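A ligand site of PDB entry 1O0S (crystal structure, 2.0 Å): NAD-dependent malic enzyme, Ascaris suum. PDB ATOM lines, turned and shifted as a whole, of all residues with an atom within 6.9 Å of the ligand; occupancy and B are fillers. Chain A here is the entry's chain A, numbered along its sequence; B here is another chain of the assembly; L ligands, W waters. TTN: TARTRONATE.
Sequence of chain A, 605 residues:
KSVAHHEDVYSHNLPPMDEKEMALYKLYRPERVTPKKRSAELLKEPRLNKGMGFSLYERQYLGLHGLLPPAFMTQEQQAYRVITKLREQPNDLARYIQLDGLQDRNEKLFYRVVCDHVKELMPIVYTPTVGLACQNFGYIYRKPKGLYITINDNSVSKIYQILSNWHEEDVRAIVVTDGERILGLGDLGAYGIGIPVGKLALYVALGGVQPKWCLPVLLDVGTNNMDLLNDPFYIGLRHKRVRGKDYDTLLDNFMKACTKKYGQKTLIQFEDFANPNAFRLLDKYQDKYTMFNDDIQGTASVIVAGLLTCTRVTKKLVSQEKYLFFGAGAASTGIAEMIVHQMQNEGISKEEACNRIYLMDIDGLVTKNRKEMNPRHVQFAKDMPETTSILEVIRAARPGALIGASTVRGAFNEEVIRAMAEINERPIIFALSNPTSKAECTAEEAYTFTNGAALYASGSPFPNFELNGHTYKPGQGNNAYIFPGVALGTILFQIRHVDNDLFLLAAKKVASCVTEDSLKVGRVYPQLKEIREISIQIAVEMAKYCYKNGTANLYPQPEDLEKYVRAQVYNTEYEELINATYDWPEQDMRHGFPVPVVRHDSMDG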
ATOM      1  N   ASN A  49     -26.794  10.949 -17.198  1.00  0.00           N
ATOM      2  CA  ASN A  49     -25.872  11.294 -16.131  1.00  0.00           C
ATOM      3  C   ASN A  49     -25.247  10.193 -15.305  1.00  0.00           C
ATOM      4  O   ASN A  49     -25.940   9.406 -14.672  1.00  0.00           O
ATOM      5  CB  ASN A  49     -26.529  12.281 -15.175  1.00  0.00           C
ATOM      6  CG  ASN A  49     -25.566  12.768 -14.142  1.00  0.00           C
ATOM      7  OD1 ASN A  49     -24.452  13.169 -14.479  1.00  0.00           O
ATOM      8  ND2 ASN A  49     -25.970  12.751 -12.874  1.00  0.00           N
ATOM      9  N   LYS A  50     -23.916  10.161 -15.296  1.00  0.00           N
ATOM     10  CA  LYS A  50     -23.156   9.177 -14.533  1.00  0.00           C
ATOM     11  C   LYS A  50     -22.549   9.843 -13.310  1.00  0.00           C
ATOM     12  O   LYS A  50     -21.980   9.163 -12.454  1.00  0.00           O
ATOM     13  CB  LYS A  50     -22.003   8.616 -15.379  1.00  0.00           C
ATOM     14  CG  LYS A  50     -22.424   7.831 -16.624  1.00  0.00           C
ATOM     15  CD  LYS A  50     -21.197   7.245 -17.361  1.00  0.00           C
ATOM     16  CE  LYS A  50     -21.527   6.876 -18.802  1.00  0.00           C
ATOM     17  NZ  LYS A  50     -20.340   6.380 -19.554  1.00  0.00           N
ATOM     18  N   GLY A  51     -22.654  11.167 -13.232  1.00  0.00           N
ATOM     19  CA  GLY A  51     -22.069  11.886 -12.109  1.00  0.00           C
ATOM     20  C   GLY A  51     -20.550  11.795 -12.145  1.00  0.00           C
ATOM     21  O   GLY A  51     -19.944  11.858 -13.214  1.00  0.00           O
ATOM     22  N   MET A  52     -19.938  11.638 -10.991  1.00  0.00           N
ATOM     23  CA  MET A  52     -18.484  11.535 -10.946  1.00  0.00           C
ATOM     24  C   MET A  52     -18.010  10.227 -11.541  1.00  0.00           C
ATOM     25  O   MET A  52     -16.812   9.915 -11.544  1.00  0.00           O
ATOM     26  CB  MET A  52     -17.974  11.692  -9.506  1.00  0.00           C
ATOM     27  CG  MET A  52     -18.172  13.095  -8.966  1.00  0.00           C
ATOM     28  SD  MET A  52     -17.687  13.284  -7.241  1.00  0.00           S
ATOM     29  CE  MET A  52     -19.128  12.552  -6.455  1.00  0.00           C
ATOM     30  N   GLY A  53     -18.957   9.446 -12.074  1.00  0.00           N
ATOM     31  CA  GLY A  53     -18.616   8.190 -12.707  1.00  0.00           C
ATOM     32  C   GLY A  53     -18.100   8.455 -14.111  1.00  0.00           C
ATOM     33  O   GLY A  53     -17.648   7.565 -14.806  1.00  0.00           O
ATOM     34  N   MET A  73     -15.052   8.260 -10.008  1.00  0.00           N
ATOM     35  CA  MET A  73     -15.489   7.034  -9.355  1.00  0.00           C
ATOM     36  C   MET A  73     -15.959   5.953 -10.304  1.00  0.00           C
ATOM     37  O   MET A  73     -16.224   6.212 -11.476  1.00  0.00           O
ATOM     38  CB  MET A  73     -16.647   7.349  -8.403  1.00  0.00           C
ATOM     39  CG  MET A  73     -16.422   8.524  -7.471  1.00  0.00           C
ATOM     40  SD  MET A  73     -17.870   8.839  -6.444  1.00  0.00           S
ATOM     41  CE  MET A  73     -17.132   9.808  -5.083  1.00  0.00           C
ATOM     42  N   THR A  74     -16.086   4.740  -9.767  1.00  0.00           N
ATOM     43  CA  THR A  74     -16.583   3.593 -10.518  1.00  0.00           C
ATOM     44  C   THR A  74     -18.026   3.539 -10.035  1.00  0.00           C
ATOM     45  O   THR A  74     -18.343   4.103  -8.985  1.00  0.00           O
ATOM     46  CB  THR A  74     -15.895   2.284 -10.106  1.00  0.00           C
ATOM     47  OG1 THR A  74     -16.022   2.118  -8.680  1.00  0.00           O
ATOM     48  CG2 THR A  74     -14.411   2.307 -10.500  1.00  0.00           C
ATOM     49  N   GLN A  77     -18.141   2.162  -6.475  1.00  0.00           N
ATOM     50  CA  GLN A  77     -17.795   3.103  -5.420  1.00  0.00           C
ATOM     51  C   GLN A  77     -18.961   4.066  -5.184  1.00  0.00           C
ATOM     52  O   GLN A  77     -19.223   4.496  -4.061  1.00  0.00           O
ATOM     53  CB  GLN A  77     -16.544   3.895  -5.813  1.00  0.00           C
ATOM     54  CG  GLN A  77     -16.396   5.238  -5.105  1.00  0.00           C
ATOM     55  CD  GLN A  77     -15.219   6.037  -5.624  1.00  0.00           C
ATOM     56  OE1 GLN A  77     -14.787   5.861  -6.764  1.00  0.00           O
ATOM     57  NE2 GLN A  77     -14.691   6.928  -4.787  1.00  0.00           N
ATOM     58  N   GLN A  78     -19.675   4.410  -6.253  1.00  0.00           N
ATOM     59  CA  GLN A  78     -20.812   5.314  -6.147  1.00  0.00           C
ATOM     60  C   GLN A  78     -21.956   4.642  -5.394  1.00  0.00           C
ATOM     61  O   GLN A  78     -22.624   5.267  -4.576  1.00  0.00           O
ATOM     62  CB  GLN A  78     -21.292   5.719  -7.541  1.00  0.00           C
ATOM     63  CG  GLN A  78     -20.570   6.930  -8.133  1.00  0.00           C
ATOM     64  CD  GLN A  78     -20.990   7.226  -9.570  1.00  0.00           C
ATOM     65  OE1 GLN A  78     -20.726   6.439 -10.479  1.00  0.00           O
ATOM     66  NE2 GLN A  78     -21.641   8.365  -9.776  1.00  0.00           N
ATOM     67  N   ALA A  79     -22.173   3.354  -5.677  1.00  0.00           N
ATOM     68  CA  ALA A  79     -23.239   2.614  -5.025  1.00  0.00           C
ATOM     69  C   ALA A  79     -22.930   2.484  -3.538  1.00  0.00           C
ATOM     70  O   ALA A  79     -23.836   2.509  -2.693  1.00  0.00           O
ATOM     71  CB  ALA A  79     -23.402   1.247  -5.658  1.00  0.00           C
ATOM     72  N   TYR A  80     -21.655   2.337  -3.214  1.00  0.00           N
ATOM     73  CA  TYR A  80     -21.238   2.227  -1.835  1.00  0.00           C
ATOM     74  C   TYR A  80     -21.632   3.513  -1.113  1.00  0.00           C
ATOM     75  O   TYR A  80     -22.239   3.471  -0.048  1.00  0.00           O
ATOM     76  CB  TYR A  80     -19.721   2.060  -1.735  1.00  0.00           C
ATOM     77  CG  TYR A  80     -19.244   1.745  -0.347  1.00  0.00           C
ATOM     78  CD1 TYR A  80     -19.220   0.434   0.123  1.00  0.00           C
ATOM     79  CD2 TYR A  80     -18.859   2.765   0.526  1.00  0.00           C
ATOM     80  CE1 TYR A  80     -18.812   0.140   1.424  1.00  0.00           C
ATOM     81  CE2 TYR A  80     -18.448   2.480   1.824  1.00  0.00           C
ATOM     82  CZ  TYR A  80     -18.430   1.172   2.263  1.00  0.00           C
ATOM     83  OH  TYR A  80     -18.022   0.884   3.551  1.00  0.00           O
ATOM     84  N   ARG A  81     -21.303   4.656  -1.710  1.00  0.00           N
ATOM     85  CA  ARG A  81     -21.620   5.955  -1.116  1.00  0.00           C
ATOM     86  C   ARG A  81     -23.123   6.096  -0.890  1.00  0.00           C
ATOM     87  O   ARG A  81     -23.566   6.602   0.142  1.00  0.00           O
ATOM     88  CB  ARG A  81     -21.129   7.111  -2.002  1.00  0.00           C
ATOM     89  CG  ARG A  81     -19.600   7.248  -2.089  1.00  0.00           C
ATOM     90  CD  ARG A  81     -19.196   8.233  -3.200  1.00  0.00           C
ATOM     91  NE  ARG A  81     -19.780   9.561  -3.025  1.00  0.00           N
ATOM     92  CZ  ARG A  81     -19.205  10.558  -2.347  1.00  0.00           C
ATOM     93  NH1 ARG A  81     -18.020  10.385  -1.788  1.00  0.00           N
ATOM     94  NH2 ARG A  81     -19.822  11.733  -2.225  1.00  0.00           N
ATOM     95  N   VAL A  82     -23.910   5.621  -1.849  1.00  0.00           N
ATOM     96  CA  VAL A  82     -25.349   5.712  -1.723  1.00  0.00           C
ATOM     97  C   VAL A  82     -25.911   4.809  -0.626  1.00  0.00           C
ATOM     98  O   VAL A  82     -26.709   5.262   0.200  1.00  0.00           O
ATOM     99  CB  VAL A  82     -26.059   5.372  -3.042  1.00  0.00           C
ATOM    100  CG1 VAL A  82     -27.578   5.255  -2.822  1.00  0.00           C
ATOM    101  CG2 VAL A  82     -25.767   6.456  -4.068  1.00  0.00           C
ATOM    102  N   LYS A  85     -25.026   6.185   2.897  1.00  0.00           N
ATOM    103  CA  LYS A  85     -25.879   7.302   3.290  1.00  0.00           C
ATOM    104  C   LYS A  85     -27.328   6.857   3.531  1.00  0.00           C
ATOM    105  O   LYS A  85     -28.046   7.426   4.358  1.00  0.00           O
ATOM    106  CB  LYS A  85     -25.833   8.412   2.240  1.00  0.00           C
ATOM    107  N   GLN A  98     -34.525  10.047  -0.409  1.00  0.00           N
ATOM    108  CA  GLN A  98     -33.170   9.964  -0.961  1.00  0.00           C
ATOM    109  C   GLN A  98     -33.162   9.137  -2.245  1.00  0.00           C
ATOM    110  O   GLN A  98     -32.462   9.465  -3.198  1.00  0.00           O
ATOM    111  CB  GLN A  98     -32.195   9.330   0.041  1.00  0.00           C
ATOM    112  CG  GLN A  98     -30.739   9.391  -0.405  1.00  0.00           C
ATOM    113  CD  GLN A  98     -29.802   8.502   0.415  1.00  0.00           C
ATOM    114  OE1 GLN A  98     -29.982   8.346   1.619  1.00  0.00           O
ATOM    115  NE2 GLN A  98     -28.797   7.936  -0.235  1.00  0.00           N
ATOM    116  N   LEU A 102     -32.350  10.042  -6.102  1.00  0.00           N
ATOM    117  CA  LEU A 102     -31.334   9.314  -6.842  1.00  0.00           C
ATOM    118  C   LEU A 102     -31.862   8.910  -8.225  1.00  0.00           C
ATOM    119  O   LEU A 102     -31.128   8.938  -9.214  1.00  0.00           O
ATOM    120  CB  LEU A 102     -30.915   8.061  -6.072  1.00  0.00           C
ATOM    121  CG  LEU A 102     -29.964   7.111  -6.807  1.00  0.00           C
ATOM    122  CD1 LEU A 102     -28.741   7.870  -7.291  1.00  0.00           C
ATOM    123  CD2 LEU A 102     -29.555   5.971  -5.895  1.00  0.00           C
ATOM    124  N   ARG A 105     -31.503  11.718 -10.436  1.00  0.00           N
ATOM    125  CA  ARG A 105     -30.126  12.161 -10.640  1.00  0.00           C
ATOM    126  C   ARG A 105     -29.265  11.308 -11.557  1.00  0.00           C
ATOM    127  O   ARG A 105     -28.676  11.805 -12.515  1.00  0.00           O
ATOM    128  CB  ARG A 105     -29.393  12.277  -9.283  1.00  0.00           C
ATOM    129  CG  ARG A 105     -27.934  12.733  -9.421  1.00  0.00           C
ATOM    130  CD  ARG A 105     -27.238  13.016  -8.085  1.00  0.00           C
ATOM    131  NE  ARG A 105     -26.823  11.804  -7.366  1.00  0.00           N
ATOM    132  CZ  ARG A 105     -27.462  11.294  -6.312  1.00  0.00           C
ATOM    133  NH1 ARG A 105     -28.548  11.885  -5.844  1.00  0.00           N
ATOM    134  NH2 ARG A 105     -26.995  10.200  -5.712  1.00  0.00           N
ATOM    135  N   ASN A 106     -29.179  10.018 -11.244  1.00  0.00           N
ATOM    136  CA  ASN A 106     -28.390   9.043 -11.980  1.00  0.00           C
ATOM    137  C   ASN A 106     -29.237   7.755 -12.032  1.00  0.00           C
ATOM    138  O   ASN A 106     -29.234   6.961 -11.098  1.00  0.00           O
ATOM    139  CB  ASN A 106     -27.091   8.806 -11.211  1.00  0.00           C
ATOM    140  CG  ASN A 106     -26.132   7.913 -11.938  1.00  0.00           C
ATOM    141  OD1 ASN A 106     -26.532   7.025 -12.682  1.00  0.00           O
ATOM    142  ND2 ASN A 106     -24.842   8.109 -11.690  1.00  0.00           N
ATOM    143  N   LEU A 109     -27.322   4.339 -11.705  1.00  0.00           N
ATOM    144  CA  LEU A 109     -26.909   4.128 -10.325  1.00  0.00           C
ATOM    145  C   LEU A 109     -28.120   3.709  -9.482  1.00  0.00           C
ATOM    146  O   LEU A 109     -28.042   2.759  -8.706  1.00  0.00           O
ATOM    147  CB  LEU A 109     -26.291   5.407  -9.765  1.00  0.00           C
ATOM    148  CG  LEU A 109     -25.717   5.253  -8.359  1.00  0.00           C
ATOM    149  CD1 LEU A 109     -24.642   4.165  -8.350  1.00  0.00           C
ATOM    150  CD2 LEU A 109     -25.142   6.585  -7.891  1.00  0.00           C
ATOM    151  N   TYR A 574     -22.922   1.282 -16.717  1.00  0.00           N
ATOM    152  CA  TYR A 574     -22.762   2.509 -17.465  1.00  0.00           C
ATOM    153  C   TYR A 574     -22.403   2.170 -18.924  1.00  0.00           C
ATOM    154  O   TYR A 574     -21.633   1.250 -19.176  1.00  0.00           O
ATOM    155  CB  TYR A 574     -21.640   3.348 -16.855  1.00  0.00           C
ATOM    156  CG  TYR A 574     -22.007   4.023 -15.550  1.00  0.00           C
ATOM    157  CD1 TYR A 574     -21.041   4.249 -14.572  1.00  0.00           C
ATOM    158  CD2 TYR A 574     -23.310   4.492 -15.324  1.00  0.00           C
ATOM    159  CE1 TYR A 574     -21.355   4.936 -13.396  1.00  0.00           C
ATOM    160  CE2 TYR A 574     -23.630   5.185 -14.137  1.00  0.00           C
ATOM    161  CZ  TYR A 574     -22.641   5.403 -13.187  1.00  0.00           C
ATOM    162  OH  TYR A 574     -22.918   6.110 -12.041  1.00  0.00           O
ATOM    163  N   TYR B 139     -20.276  16.443  -0.502  1.00  0.00           N
ATOM    164  CA  TYR B 139     -20.813  16.639  -1.843  1.00  0.00           C
ATOM    165  C   TYR B 139     -22.310  16.471  -1.838  1.00  0.00           C
ATOM    166  O   TYR B 139     -22.828  15.361  -1.939  1.00  0.00           O
ATOM    167  CB  TYR B 139     -20.191  15.651  -2.841  1.00  0.00           C
ATOM    168  CG  TYR B 139     -20.701  15.829  -4.264  1.00  0.00           C
ATOM    169  CD1 TYR B 139     -20.582  17.045  -4.930  1.00  0.00           C
ATOM    170  CD2 TYR B 139     -21.299  14.762  -4.941  1.00  0.00           C
ATOM    171  CE1 TYR B 139     -21.039  17.198  -6.237  1.00  0.00           C
ATOM    172  CE2 TYR B 139     -21.752  14.909  -6.260  1.00  0.00           C
ATOM    173  CZ  TYR B 139     -21.623  16.131  -6.898  1.00  0.00           C
ATOM    174  OH  TYR B 139     -22.051  16.273  -8.203  1.00  0.00           O
ATOM    175  N   TYR B 141     -26.112  16.841  -3.295  1.00  0.00           N
ATOM    176  CA  TYR B 141     -26.691  16.673  -4.621  1.00  0.00           C
ATOM    177  C   TYR B 141     -27.463  17.918  -5.054  1.00  0.00           C
ATOM    178  O   TYR B 141     -28.317  18.419  -4.316  1.00  0.00           O
ATOM    179  CB  TYR B 141     -27.652  15.496  -4.622  1.00  0.00           C
ATOM    180  CG  TYR B 141     -27.163  14.319  -3.818  1.00  0.00           C
ATOM    181  CD1 TYR B 141     -27.586  14.123  -2.495  1.00  0.00           C
ATOM    182  CD2 TYR B 141     -26.298  13.378  -4.371  1.00  0.00           C
ATOM    183  CE1 TYR B 141     -27.161  13.031  -1.750  1.00  0.00           C
ATOM    184  CE2 TYR B 141     -25.865  12.288  -3.641  1.00  0.00           C
ATOM    185  CZ  TYR B 141     -26.292  12.112  -2.332  1.00  0.00           C
ATOM    186  OH  TYR B 141     -25.875  11.016  -1.605  1.00  0.00           O
ATOM    187  N   PHE B 233     -14.663   9.632   1.494  1.00  0.00           N
ATOM    188  CA  PHE B 233     -15.808  10.270   0.846  1.00  0.00           C
ATOM    189  C   PHE B 233     -15.505  11.663   0.283  1.00  0.00           C
ATOM    190  O   PHE B 233     -16.331  12.254  -0.417  1.00  0.00           O
ATOM    191  CB  PHE B 233     -16.985  10.352   1.822  1.00  0.00           C
ATOM    192  CG  PHE B 233     -17.656   9.031   2.070  1.00  0.00           C
ATOM    193  CD1 PHE B 233     -16.986   8.012   2.732  1.00  0.00           C
ATOM    194  CD2 PHE B 233     -18.938   8.800   1.609  1.00  0.00           C
ATOM    195  CE1 PHE B 233     -17.594   6.773   2.929  1.00  0.00           C
ATOM    196  CE2 PHE B 233     -19.554   7.572   1.797  1.00  0.00           C
ATOM    197  CZ  PHE B 233     -18.884   6.554   2.458  1.00  0.00           C
ATOM    198  N   ILE B 235     -14.215  14.548  -2.078  1.00  0.00           N
ATOM    199  CA  ILE B 235     -14.224  14.552  -3.540  1.00  0.00           C
ATOM    200  C   ILE B 235     -13.399  15.636  -4.240  1.00  0.00           C
ATOM    201  O   ILE B 235     -13.648  15.948  -5.406  1.00  0.00           O
ATOM    202  CB  ILE B 235     -15.687  14.589  -4.066  1.00  0.00           C
ATOM    203  CG1 ILE B 235     -16.507  15.623  -3.299  1.00  0.00           C
ATOM    204  CG2 ILE B 235     -16.342  13.236  -3.828  1.00  0.00           C
ATOM    205  CD1 ILE B 235     -16.106  17.061  -3.528  1.00  0.00           C
HETATM  206  C1  TTN L   1     -23.196   9.675  -6.662  1.00  0.00           C
HETATM  207  C2  TTN L   1     -22.900   8.960  -5.330  1.00  0.00           C
HETATM  208  C3  TTN L   1     -23.340   9.840  -4.171  1.00  0.00           C
HETATM  209  O1  TTN L   1     -24.363   9.962  -6.980  1.00  0.00           O
HETATM  210  O2  TTN L   1     -22.267   9.975  -7.432  1.00  0.00           O
HETATM  211  O3  TTN L   1     -21.484   8.702  -5.218  1.00  0.00           O
HETATM  212  O4  TTN L   1     -24.504   9.760  -3.763  1.00  0.00           O
HETATM  213  O5  TTN L   1     -22.541  10.625  -3.639  1.00  0.00           O
HETATM  214  O   HOH W   1     -23.266  13.361  -3.510  1.00  0.00           O
HETATM  215  O   HOH W   2     -21.400  11.968  -8.759  1.00  0.00           O
HETATM  216  O   HOH W   3     -24.519  10.572  -9.783  1.00  0.00           O
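NE of Arg 81 lies within salt-bridge range of O5 of the ligand, at 3.0 Å. An oxygen (O4) of the ligand is in hydrogen-bond range of the side-chain hydroxyl (OH) of Tyr 141 of chain B (2.8 Å). The guanidinium group (NH2) of Arg 105 is in salt-bridge range of an oxygen (O1) of the ligand (2.9 Å). The side-chain amide nitrogen (NE2) of Gln 78 sits at hydrogen-bond distance from an oxygen (O2) of the ligand (2.9 Å).
OE1 of Gln 78 lies within hydrogen-bond range of OH of Tyr 574 (2.7 Å). The backbone carbonyl oxygen (O) of Arg 105 sits at hydrogen-bond distance from the side-chain amide nitrogen (ND2) of Asn 49. NE2 of Gln 78 is in hydrogen-bond range of O of Lys 50, 2.8 Å away. O of Phe 233 of chain B lies within hydrogen-bond range of NH1 of Arg 81, 2.9 Å away. The backbone NH (N) of Leu 109 sits at hydrogen-bond distance from the side-chain amide oxygen (OD1) of Asn 106 (3.0 Å). The backbone carbonyl oxygen of Val 82 sits at hydrogen-bond distance from the side-chain amide nitrogen of Gln 98 (3.4 Å). The backbone carbonyl oxygen (O) of Met 52 lies within hydrogen-bond range of the backbone NH (N) of Met 73, at 2.9 Å.
Residues that only touch the ligand: Val 82, Leu 109 and Met 73. Along chain A the residues within 4 Å of the ligand span positions 73 to 109.
Water W2 lies within hydrogen-bond range of O2 of the ligand and N of Met 52. Water W1 lies within hydrogen-bond range of the backbone carbonyl oxygen of Tyr 139 of chain B (2.6 Å) and an oxygen (O5) of the ligand (2.8 Å). Water W3 lies within hydrogen-bond range of O1 of the ligand and ND2 of Asn 106.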
